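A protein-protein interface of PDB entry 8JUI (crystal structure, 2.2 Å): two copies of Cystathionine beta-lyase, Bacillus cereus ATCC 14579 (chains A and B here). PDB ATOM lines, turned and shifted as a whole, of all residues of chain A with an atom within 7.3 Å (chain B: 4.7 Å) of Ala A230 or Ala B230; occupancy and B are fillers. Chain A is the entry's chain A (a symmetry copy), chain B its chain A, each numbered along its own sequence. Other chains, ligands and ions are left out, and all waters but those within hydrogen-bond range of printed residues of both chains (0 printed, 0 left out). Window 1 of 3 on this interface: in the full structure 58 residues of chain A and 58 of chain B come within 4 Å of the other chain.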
ATOM      1  N   ARG A  48      16.928  -1.497   9.918  1.00  0.00           N
ATOM      2  CA  ARG A  48      16.201  -2.312   8.909  1.00  0.00           C
ATOM      3  C   ARG A  48      14.742  -2.539   9.367  1.00  0.00           C
ATOM      4  O   ARG A  48      13.844  -2.352   8.548  1.00  0.00           O
ATOM      5  CB  ARG A  48      16.952  -3.619   8.598  1.00  0.00           C
ATOM      6  CG  ARG A  48      16.226  -4.475   7.564  1.00  0.00           C
ATOM      7  CD  ARG A  48      17.108  -5.517   6.904  1.00  0.00           C
ATOM      8  NE  ARG A  48      17.923  -6.266   7.858  1.00  0.00           N
ATOM      9  CZ  ARG A  48      17.476  -7.260   8.632  1.00  0.00           C
ATOM     10  NH1 ARG A  48      18.310  -7.887   9.449  1.00  0.00           N
ATOM     11  NH2 ARG A  48      16.198  -7.622   8.591  1.00  0.00           N
ATOM     12  N   ALA A  72       8.608   1.941   2.561  1.00  0.00           N
ATOM     13  CA  ALA A  72       9.699   2.531   1.769  1.00  0.00           C
ATOM     14  C   ALA A  72      10.752   1.466   1.421  1.00  0.00           C
ATOM     15  O   ALA A  72      11.290   0.757   2.349  1.00  0.00           O
ATOM     16  CB  ALA A  72      10.302   3.692   2.517  1.00  0.00           C
ATOM     17  N   PHE A  73      11.114   1.410   0.142  1.00  0.00           N
ATOM     18  CA  PHE A  73      12.027   0.384  -0.411  1.00  0.00           C
ATOM     19  C   PHE A  73      13.199   1.019  -1.153  1.00  0.00           C
ATOM     20  O   PHE A  73      13.123   2.161  -1.566  1.00  0.00           O
ATOM     21  CB  PHE A  73      11.284  -0.540  -1.365  1.00  0.00           C
ATOM     22  CG  PHE A  73      10.194  -1.354  -0.737  1.00  0.00           C
ATOM     23  CD1 PHE A  73       8.904  -0.862  -0.657  1.00  0.00           C
ATOM     24  CD2 PHE A  73      10.443  -2.637  -0.283  1.00  0.00           C
ATOM     25  CE1 PHE A  73       7.886  -1.620  -0.101  1.00  0.00           C
ATOM     26  CE2 PHE A  73       9.424  -3.396   0.277  1.00  0.00           C
ATOM     27  CZ  PHE A  73       8.152  -2.880   0.375  1.00  0.00           C
ATOM     28  N   ALA A  74      14.251   0.245  -1.331  1.00  0.00           N
ATOM     29  CA  ALA A  74      15.517   0.652  -1.995  1.00  0.00           C
ATOM     30  C   ALA A  74      15.290   1.141  -3.436  1.00  0.00           C
ATOM     31  O   ALA A  74      16.141   1.913  -3.963  1.00  0.00           O
ATOM     32  CB  ALA A  74      16.487  -0.486  -1.947  1.00  0.00           C
ATOM     33  N   SER A  75      14.148   0.806  -4.038  1.00  0.00           N
ATOM     34  CA  SER A  75      13.870   1.151  -5.449  1.00  0.00           C
ATOM     35  C   SER A  75      12.391   0.883  -5.698  1.00  0.00           C
ATOM     36  O   SER A  75      11.809   0.107  -4.950  1.00  0.00           O
ATOM     37  CB  SER A  75      14.805   0.350  -6.396  1.00  0.00           C
ATOM     38  OG  SER A  75      14.432  -1.042  -6.459  1.00  0.00           O
ATOM     39  N   ILE A  77      11.290  -0.904  -8.207  1.00  0.00           N
ATOM     40  CA  ILE A  77      11.213  -2.347  -8.598  1.00  0.00           C
ATOM     41  C   ILE A  77      11.326  -3.225  -7.344  1.00  0.00           C
ATOM     42  O   ILE A  77      10.677  -4.264  -7.335  1.00  0.00           O
ATOM     43  CB  ILE A  77      12.206  -2.741  -9.704  1.00  0.00           C
ATOM     44  CG1 ILE A  77      11.817  -4.068 -10.378  1.00  0.00           C
ATOM     45  CG2 ILE A  77      13.623  -2.804  -9.194  1.00  0.00           C
ATOM     46  CD1 ILE A  77      10.423  -4.098 -10.941  1.00  0.00           C
ATOM     47  N   ALA A  78      12.029  -2.807  -6.288  1.00  0.00           N
ATOM     48  CA  ALA A  78      12.072  -3.593  -5.023  1.00  0.00           C
ATOM     49  C   ALA A  78      10.712  -3.573  -4.338  1.00  0.00           C
ATOM     50  O   ALA A  78      10.356  -4.618  -3.742  1.00  0.00           O
ATOM     51  CB  ALA A  78      13.144  -3.128  -4.066  1.00  0.00           C
ATOM     52  N   ALA A  79       9.986  -2.443  -4.396  1.00  0.00           N
ATOM     53  CA  ALA A  79       8.618  -2.341  -3.854  1.00  0.00           C
ATOM     54  C   ALA A  79       7.700  -3.297  -4.622  1.00  0.00           C
ATOM     55  O   ALA A  79       6.854  -3.935  -4.003  1.00  0.00           O
ATOM     56  CB  ALA A  79       8.062  -0.940  -3.902  1.00  0.00           C
ATOM     57  N   THR A  82       8.720  -6.956  -3.893  1.00  0.00           N
ATOM     58  CA  THR A  82       8.309  -7.356  -2.525  1.00  0.00           C
ATOM     59  C   THR A  82       6.801  -7.610  -2.537  1.00  0.00           C
ATOM     60  O   THR A  82       6.367  -8.589  -1.938  1.00  0.00           O
ATOM     61  CB  THR A  82       8.757  -6.358  -1.455  1.00  0.00           C
ATOM     62  OG1 THR A  82      10.175  -6.150  -1.510  1.00  0.00           O
ATOM     63  CG2 THR A  82       8.366  -6.790  -0.064  1.00  0.00           C
ATOM     64  N   GLY A 208      11.523   3.284  -3.722  1.00  0.00           N
ATOM     65  CA  GLY A 208      10.163   2.761  -3.969  1.00  0.00           C
ATOM     66  C   GLY A 208       9.223   2.933  -2.777  1.00  0.00           C
ATOM     67  O   GLY A 208       9.682   2.905  -1.668  1.00  0.00           O
ATOM     68  N   LEU A 224       7.206  -8.840   4.798  1.00  0.00           N
ATOM     69  CA  LEU A 224       8.069  -9.077   3.615  1.00  0.00           C
ATOM     70  C   LEU A 224       9.118  -7.963   3.471  1.00  0.00           C
ATOM     71  O   LEU A 224      10.249  -8.271   3.008  1.00  0.00           O
ATOM     72  CB  LEU A 224       7.191  -9.241   2.367  1.00  0.00           C
ATOM     73  CG  LEU A 224       6.375 -10.532   2.330  1.00  0.00           C
ATOM     74  CD1 LEU A 224       5.218 -10.440   1.363  1.00  0.00           C
ATOM     75  CD2 LEU A 224       7.267 -11.720   2.010  1.00  0.00           C
ATOM     76  N   GLN A 225       8.774  -6.708   3.787  1.00  0.00           N
ATOM     77  CA  GLN A 225       9.735  -5.552   3.718  1.00  0.00           C
ATOM     78  C   GLN A 225      10.949  -5.895   4.599  1.00  0.00           C
ATOM     79  O   GLN A 225      12.113  -5.873   4.115  1.00  0.00           O
ATOM     80  CB  GLN A 225       9.077  -4.267   4.234  1.00  0.00           C
ATOM     81  CG  GLN A 225       9.911  -3.007   4.016  1.00  0.00           C
ATOM     82  CD  GLN A 225       9.396  -1.847   4.822  1.00  0.00           C
ATOM     83  OE1 GLN A 225       8.697  -2.051   5.798  1.00  0.00           O
ATOM     84  NE2 GLN A 225       9.810  -0.637   4.480  1.00  0.00           N
ATOM     85  N   ASN A 226      10.673  -6.249   5.846  1.00  0.00           N
ATOM     86  CA  ASN A 226      11.711  -6.625   6.846  1.00  0.00           C
ATOM     87  C   ASN A 226      12.428  -7.904   6.395  1.00  0.00           C
ATOM     88  O   ASN A 226      13.657  -7.906   6.457  1.00  0.00           O
ATOM     89  CB  ASN A 226      11.148  -6.685   8.278  1.00  0.00           C
ATOM     90  CG  ASN A 226      12.247  -6.856   9.317  1.00  0.00           C
ATOM     91  OD1 ASN A 226      13.066  -5.957   9.510  1.00  0.00           O
ATOM     92  ND2 ASN A 226      12.330  -8.020   9.952  1.00  0.00           N
ATOM     93  N   ALA A 227      11.714  -8.941   5.929  1.00  0.00           N
ATOM     94  CA  ALA A 227      12.270 -10.309   5.734  1.00  0.00           C
ATOM     95  C   ALA A 227      13.216 -10.353   4.527  1.00  0.00           C
ATOM     96  O   ALA A 227      14.283 -10.954   4.610  1.00  0.00           O
ATOM     97  CB  ALA A 227      11.162 -11.342   5.583  1.00  0.00           C
ATOM     98  N   PHE A 228      12.839  -9.731   3.421  1.00  0.00           N
ATOM     99  CA  PHE A 228      13.713  -9.631   2.239  1.00  0.00           C
ATOM    100  C   PHE A 228      14.733  -8.500   2.439  1.00  0.00           C
ATOM    101  O   PHE A 228      15.862  -8.650   1.991  1.00  0.00           O
ATOM    102  CB  PHE A 228      12.868  -9.459   0.984  1.00  0.00           C
ATOM    103  CG  PHE A 228      13.600  -9.937  -0.225  1.00  0.00           C
ATOM    104  CD1 PHE A 228      14.606  -9.149  -0.779  1.00  0.00           C
ATOM    105  CD2 PHE A 228      13.355 -11.196  -0.749  1.00  0.00           C
ATOM    106  CE1 PHE A 228      15.317  -9.592  -1.881  1.00  0.00           C
ATOM    107  CE2 PHE A 228      14.068 -11.638  -1.859  1.00  0.00           C
ATOM    108  CZ  PHE A 228      15.056 -10.846  -2.402  1.00  0.00           C
ATOM    109  N   GLY A 229      14.343  -7.399   3.074  1.00  0.00           N
ATOM    110  CA  GLY A 229      15.263  -6.359   3.581  1.00  0.00           C
ATOM    111  C   GLY A 229      15.637  -5.306   2.544  1.00  0.00           C
ATOM    112  O   GLY A 229      16.733  -4.680   2.692  1.00  0.00           O
ATOM    113  N   ALA A 230      14.766  -5.054   1.561  1.00  0.00           N
ATOM    114  CA  ALA A 230      15.058  -4.157   0.424  1.00  0.00           C
ATOM    115  C   ALA A 230      14.612  -2.746   0.831  1.00  0.00           C
ATOM    116  O   ALA A 230      13.748  -2.131   0.155  1.00  0.00           O
ATOM    117  CB  ALA A 230      14.405  -4.687  -0.824  1.00  0.00           C
ATOM    118  N   ILE A 231      15.131  -2.296   1.974  1.00  0.00           N
ATOM    119  CA  ILE A 231      14.655  -1.076   2.671  1.00  0.00           C
ATOM    120  C   ILE A 231      15.351   0.147   2.086  1.00  0.00           C
ATOM    121  O   ILE A 231      16.496   0.040   1.610  1.00  0.00           O
ATOM    122  CB  ILE A 231      14.915  -1.132   4.185  1.00  0.00           C
ATOM    123  CG1 ILE A 231      16.404  -1.399   4.470  1.00  0.00           C
ATOM    124  CG2 ILE A 231      13.977  -2.154   4.827  1.00  0.00           C
ATOM    125  CD1 ILE A 231      16.832  -0.999   5.842  1.00  0.00           C
ATOM    126  N   LEU A 232      14.682   1.284   2.205  1.00  0.00           N
ATOM    127  CA  LEU A 232      15.250   2.581   1.831  1.00  0.00           C
ATOM    128  C   LEU A 232      16.063   3.041   3.042  1.00  0.00           C
ATOM    129  O   LEU A 232      15.506   3.078   4.161  1.00  0.00           O
ATOM    130  CB  LEU A 232      14.128   3.559   1.457  1.00  0.00           C
ATOM    131  CG  LEU A 232      14.609   4.875   0.820  1.00  0.00           C
ATOM    132  CD1 LEU A 232      15.340   4.633  -0.519  1.00  0.00           C
ATOM    133  CD2 LEU A 232      13.436   5.821   0.604  1.00  0.00           C
ATOM    134  N   GLY A 233      17.326   3.362   2.813  1.00  0.00           N
ATOM    135  CA  GLY A 233      18.208   3.930   3.852  1.00  0.00           C
ATOM    136  C   GLY A 233      17.730   5.312   4.310  1.00  0.00           C
ATOM    137  O   GLY A 233      17.094   6.060   3.568  1.00  0.00           O
ATOM    138  N   ALA B  72      26.619  -5.034  -4.124  1.00  0.00           N
ATOM    139  CA  ALA B  72      26.204  -4.240  -2.956  1.00  0.00           C
ATOM    140  C   ALA B  72      24.671  -4.160  -2.876  1.00  0.00           C
ATOM    141  O   ALA B  72      23.988  -3.746  -3.884  1.00  0.00           O
ATOM    142  CB  ALA B  72      26.834  -2.873  -3.019  1.00  0.00           C
ATOM    143  N   PHE B  73      24.139  -4.449  -1.691  1.00  0.00           N
ATOM    144  CA  PHE B  73      22.683  -4.537  -1.440  1.00  0.00           C
ATOM    145  C   PHE B  73      22.259  -3.639  -0.282  1.00  0.00           C
ATOM    146  O   PHE B  73      23.074  -3.268   0.542  1.00  0.00           O
ATOM    147  CB  PHE B  73      22.276  -5.969  -1.126  1.00  0.00           C
ATOM    148  CG  PHE B  73      22.492  -6.947  -2.241  1.00  0.00           C
ATOM    149  CD1 PHE B  73      23.696  -7.616  -2.368  1.00  0.00           C
ATOM    150  CD2 PHE B  73      21.471  -7.247  -3.124  1.00  0.00           C
ATOM    151  CE1 PHE B  73      23.893  -8.541  -3.382  1.00  0.00           C
ATOM    152  CE2 PHE B  73      21.667  -8.171  -4.141  1.00  0.00           C
ATOM    153  CZ  PHE B  73      22.882  -8.807  -4.272  1.00  0.00           C
ATOM    154  N   ALA B  74      20.977  -3.336  -0.232  1.00  0.00           N
ATOM    155  CA  ALA B  74      20.340  -2.456   0.782  1.00  0.00           C
ATOM    156  C   ALA B  74      20.557  -2.964   2.217  1.00  0.00           C
ATOM    157  O   ALA B  74      20.483  -2.145   3.175  1.00  0.00           O
ATOM    158  CB  ALA B  74      18.885  -2.311   0.464  1.00  0.00           C
ATOM    159  N   ALA B  78      19.121  -8.642   2.455  1.00  0.00           N
ATOM    160  CA  ALA B  78      18.764  -8.498   1.016  1.00  0.00           C
ATOM    161  C   ALA B  78      19.784  -9.216   0.142  1.00  0.00           C
ATOM    162  O   ALA B  78      19.354  -9.782  -0.892  1.00  0.00           O
ATOM    163  CB  ALA B  78      18.621  -7.061   0.576  1.00  0.00           C
ATOM    164  N   THR B  82      18.625 -12.289  -2.056  1.00  0.00           N
ATOM    165  CA  THR B  82      18.866 -12.237  -3.519  1.00  0.00           C
ATOM    166  C   THR B  82      19.635 -13.499  -3.918  1.00  0.00           C
ATOM    167  O   THR B  82      19.304 -14.086  -4.943  1.00  0.00           O
ATOM    168  CB  THR B  82      19.539 -10.939  -3.965  1.00  0.00           C
ATOM    169  OG1 THR B  82      18.780  -9.797  -3.543  1.00  0.00           O
ATOM    170  CG2 THR B  82      19.747 -10.880  -5.457  1.00  0.00           C
ATOM    171  N   GLN B 225      20.327  -8.939  -8.760  1.00  0.00           N
ATOM    172  CA  GLN B 225      20.561  -7.647  -8.026  1.00  0.00           C
ATOM    173  C   GLN B 225      19.710  -6.559  -8.704  1.00  0.00           C
ATOM    174  O   GLN B 225      18.888  -5.882  -8.031  1.00  0.00           O
ATOM    175  CB  GLN B 225      22.040  -7.248  -8.085  1.00  0.00           C
ATOM    176  CG  GLN B 225      22.402  -6.058  -7.201  1.00  0.00           C
ATOM    177  CD  GLN B 225      23.756  -5.499  -7.541  1.00  0.00           C
ATOM    178  OE1 GLN B 225      24.247  -5.721  -8.632  1.00  0.00           O
ATOM    179  NE2 GLN B 225      24.324  -4.697  -6.652  1.00  0.00           N
ATOM    180  N   PHE B 228      15.414  -7.653  -8.865  1.00  0.00           N
ATOM    181  CA  PHE B 228      14.694  -7.439  -7.598  1.00  0.00           C
ATOM    182  C   PHE B 228      14.926  -6.003  -7.100  1.00  0.00           C
ATOM    183  O   PHE B 228      14.005  -5.429  -6.537  1.00  0.00           O
ATOM    184  CB  PHE B 228      15.107  -8.497  -6.583  1.00  0.00           C
ATOM    185  CG  PHE B 228      14.040  -8.703  -5.560  1.00  0.00           C
ATOM    186  CD1 PHE B 228      13.874  -7.771  -4.539  1.00  0.00           C
ATOM    187  CD2 PHE B 228      13.154  -9.763  -5.665  1.00  0.00           C
ATOM    188  CE1 PHE B 228      12.868  -7.930  -3.600  1.00  0.00           C
ATOM    189  CE2 PHE B 228      12.147  -9.924  -4.720  1.00  0.00           C
ATOM    190  CZ  PHE B 228      11.997  -8.998  -3.709  1.00  0.00           C
ATOM    191  N   GLY B 229      16.122  -5.454  -7.288  1.00  0.00           N
ATOM    192  CA  GLY B 229      16.411  -4.014  -7.121  1.00  0.00           C
ATOM    193  C   GLY B 229      16.748  -3.613  -5.689  1.00  0.00           C
ATOM    194  O   GLY B 229      16.545  -2.408  -5.341  1.00  0.00           O
ATOM    195  N   ALA B 230      17.292  -4.534  -4.889  1.00  0.00           N
ATOM    196  CA  ALA B 230      17.542  -4.318  -3.449  1.00  0.00           C
ATOM    197  C   ALA B 230      18.959  -3.742  -3.317  1.00  0.00           C
ATOM    198  O   ALA B 230      19.831  -4.340  -2.636  1.00  0.00           O
ATOM    199  CB  ALA B 230      17.312  -5.598  -2.692  1.00  0.00           C
ATOM    200  N   ILE B 231      19.194  -2.646  -4.040  1.00  0.00           N
ATOM    201  CA  ILE B 231      20.546  -2.072  -4.249  1.00  0.00           C
ATOM    202  C   ILE B 231      20.894  -1.154  -3.083  1.00  0.00           C
ATOM    203  O   ILE B 231      19.989  -0.555  -2.474  1.00  0.00           O
ATOM    204  CB  ILE B 231      20.644  -1.281  -5.564  1.00  0.00           C
ATOM    205  CG1 ILE B 231      19.554  -0.196  -5.626  1.00  0.00           C
ATOM    206  CG2 ILE B 231      20.611  -2.250  -6.747  1.00  0.00           C
ATOM    207  CD1 ILE B 231      19.857   0.901  -6.593  1.00  0.00           C
ATOM    208  N   LEU B 232      22.190  -1.007  -2.854  1.00  0.00           N
ATOM    209  CA  LEU B 232      22.718  -0.059  -1.870  1.00  0.00           C
ATOM    210  C   LEU B 232      22.787   1.289  -2.590  1.00  0.00           C
ATOM    211  O   LEU B 232      23.395   1.358  -3.680  1.00  0.00           O
ATOM    212  CB  LEU B 232      24.085  -0.535  -1.360  1.00  0.00           C
ATOM    213  CG  LEU B 232      24.629   0.249  -0.152  1.00  0.00           C
ATOM    214  CD1 LEU B 232      23.712   0.112   1.083  1.00  0.00           C
ATOM    215  CD2 LEU B 232      26.036  -0.216   0.194  1.00  0.00           C
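OG of Ser A75 lies within hydrogen-bond range of O of Gly B229, 2.8 Å away.
N of Ala A78 sits close to O of Phe B228 (3.3 Å).
O of Phe A228 sits close to N of Ala B78 (3.3 Å).
O of Ala A78 lies within hydrogen-bond range of OG1 of Thr A82.
N of Ala A74 is in hydrogen-bond range of O of Ala A230, at 2.8 Å.
The backbone NH (N) of Ala B74 sits at hydrogen-bond distance from the backbone carbonyl oxygen (O) of Ala B230, at 2.8 Å.
The side-chain hydroxyl (OG1) of Thr B82 lies within hydrogen-bond range of the backbone carbonyl oxygen (O) of Ala B78, at 2.7 Å.
The side-chain hydroxyl of Ser A75 sits at hydrogen-bond distance from the backbone NH of Ala A78.
The backbone carbonyl oxygen of Ser A75 lies close to the backbone NH of Gly A208.
Among the printed residues, merely in contact across the chains: Phe A228 with Phe B228 (3.4 Å), Ala A74 with Ile B231 (3.5 Å), Ile A231 with Ala B74 (3.5 Å), Ile A77 with Phe B228 (3.6 Å), Ala A230 with Ala B230 (3.6 Å), Ile A77 with Gly B229 (3.7 Å), Ala A78 with Gly B229 (3.7 Å), Gly A229 with Ala B78 (3.7 Å), Thr A82 with Phe B228 (3.8 Å), Phe A228 with Thr B82 (3.8 Å), Ala A74 with Ala B74 (3.9 Å), Gly A229 with Ala B74 (3.9 Å) and Ala A74 with Gly B229 (3.9 Å).
Of chain B, only Ala B230 (3.6 Å) comes within 4 Å of Ala A230.
Of chain A, only Ala A230 comes within 4 Å of Ala B230.
Of chain A, only Ala A74 (3.9 Å), Ser A75 (2.8 Å), Ile A77 (3.7 Å) and Ala A78 (3.7 Å) come within 4 Å of Gly B229.
Of the printed residues of chain B, Thr A82 touches Phe B228 (3.8 Å).
Printed residues of chain A within 4 Å of Ala B74: Ala A74 (3.9 Å), Gly A229 (3.9 Å) and Ile A231 (3.5 Å).
Of the printed residues of chain B, Ala A78 touches Phe B228 and Gly B229.
Printed residues of chain B within 4 Å of Ile A77: Phe B228 (3.6 Å) and Gly B229 (3.7 Å).
The nearest residue of chain B that does not touch Ala A230 is Ala B74 (4.2 Å).
The nearest printed residue of chain A that does not touch Thr B82 is Ala A230 (7.3 Å).
Of the 20 printed residues of chain A, 9 touch a printed residue of chain B.
Printed residues of chain B that touch a printed residue of chain A: Ala B74, Ala B78, Thr B82, Phe B228, Gly B229, Ala B230 and Ile B231.
Hydrophobic or aromatic side chains of chain B within 4 Å of the printed part of chain A: Ala B74, Ala B78, Phe B228 and Ala B230.
Along chain B the printed residues that touch a printed residue of chain A span positions 74 to 231.
Among the printed residues, no Asp or Glu carboxylate lies within 4 Å of a Lys or Arg side-chain nitrogen of the other chain.
Ala A74 touches Gly B229, and with the chains exchanged Gly A229 touches Ala B74.
Ala A78 touches Phe B228, and with the chains exchanged Phe A228 touches Ala B78.
Phe B228 touches its own counterpart, Phe A228.
Ala A230 touches its own counterpart, Ala B230.
Of the 16 pairs that touch across the chains among the printed residues, 13 have their exchanged pair printed and touching as well.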
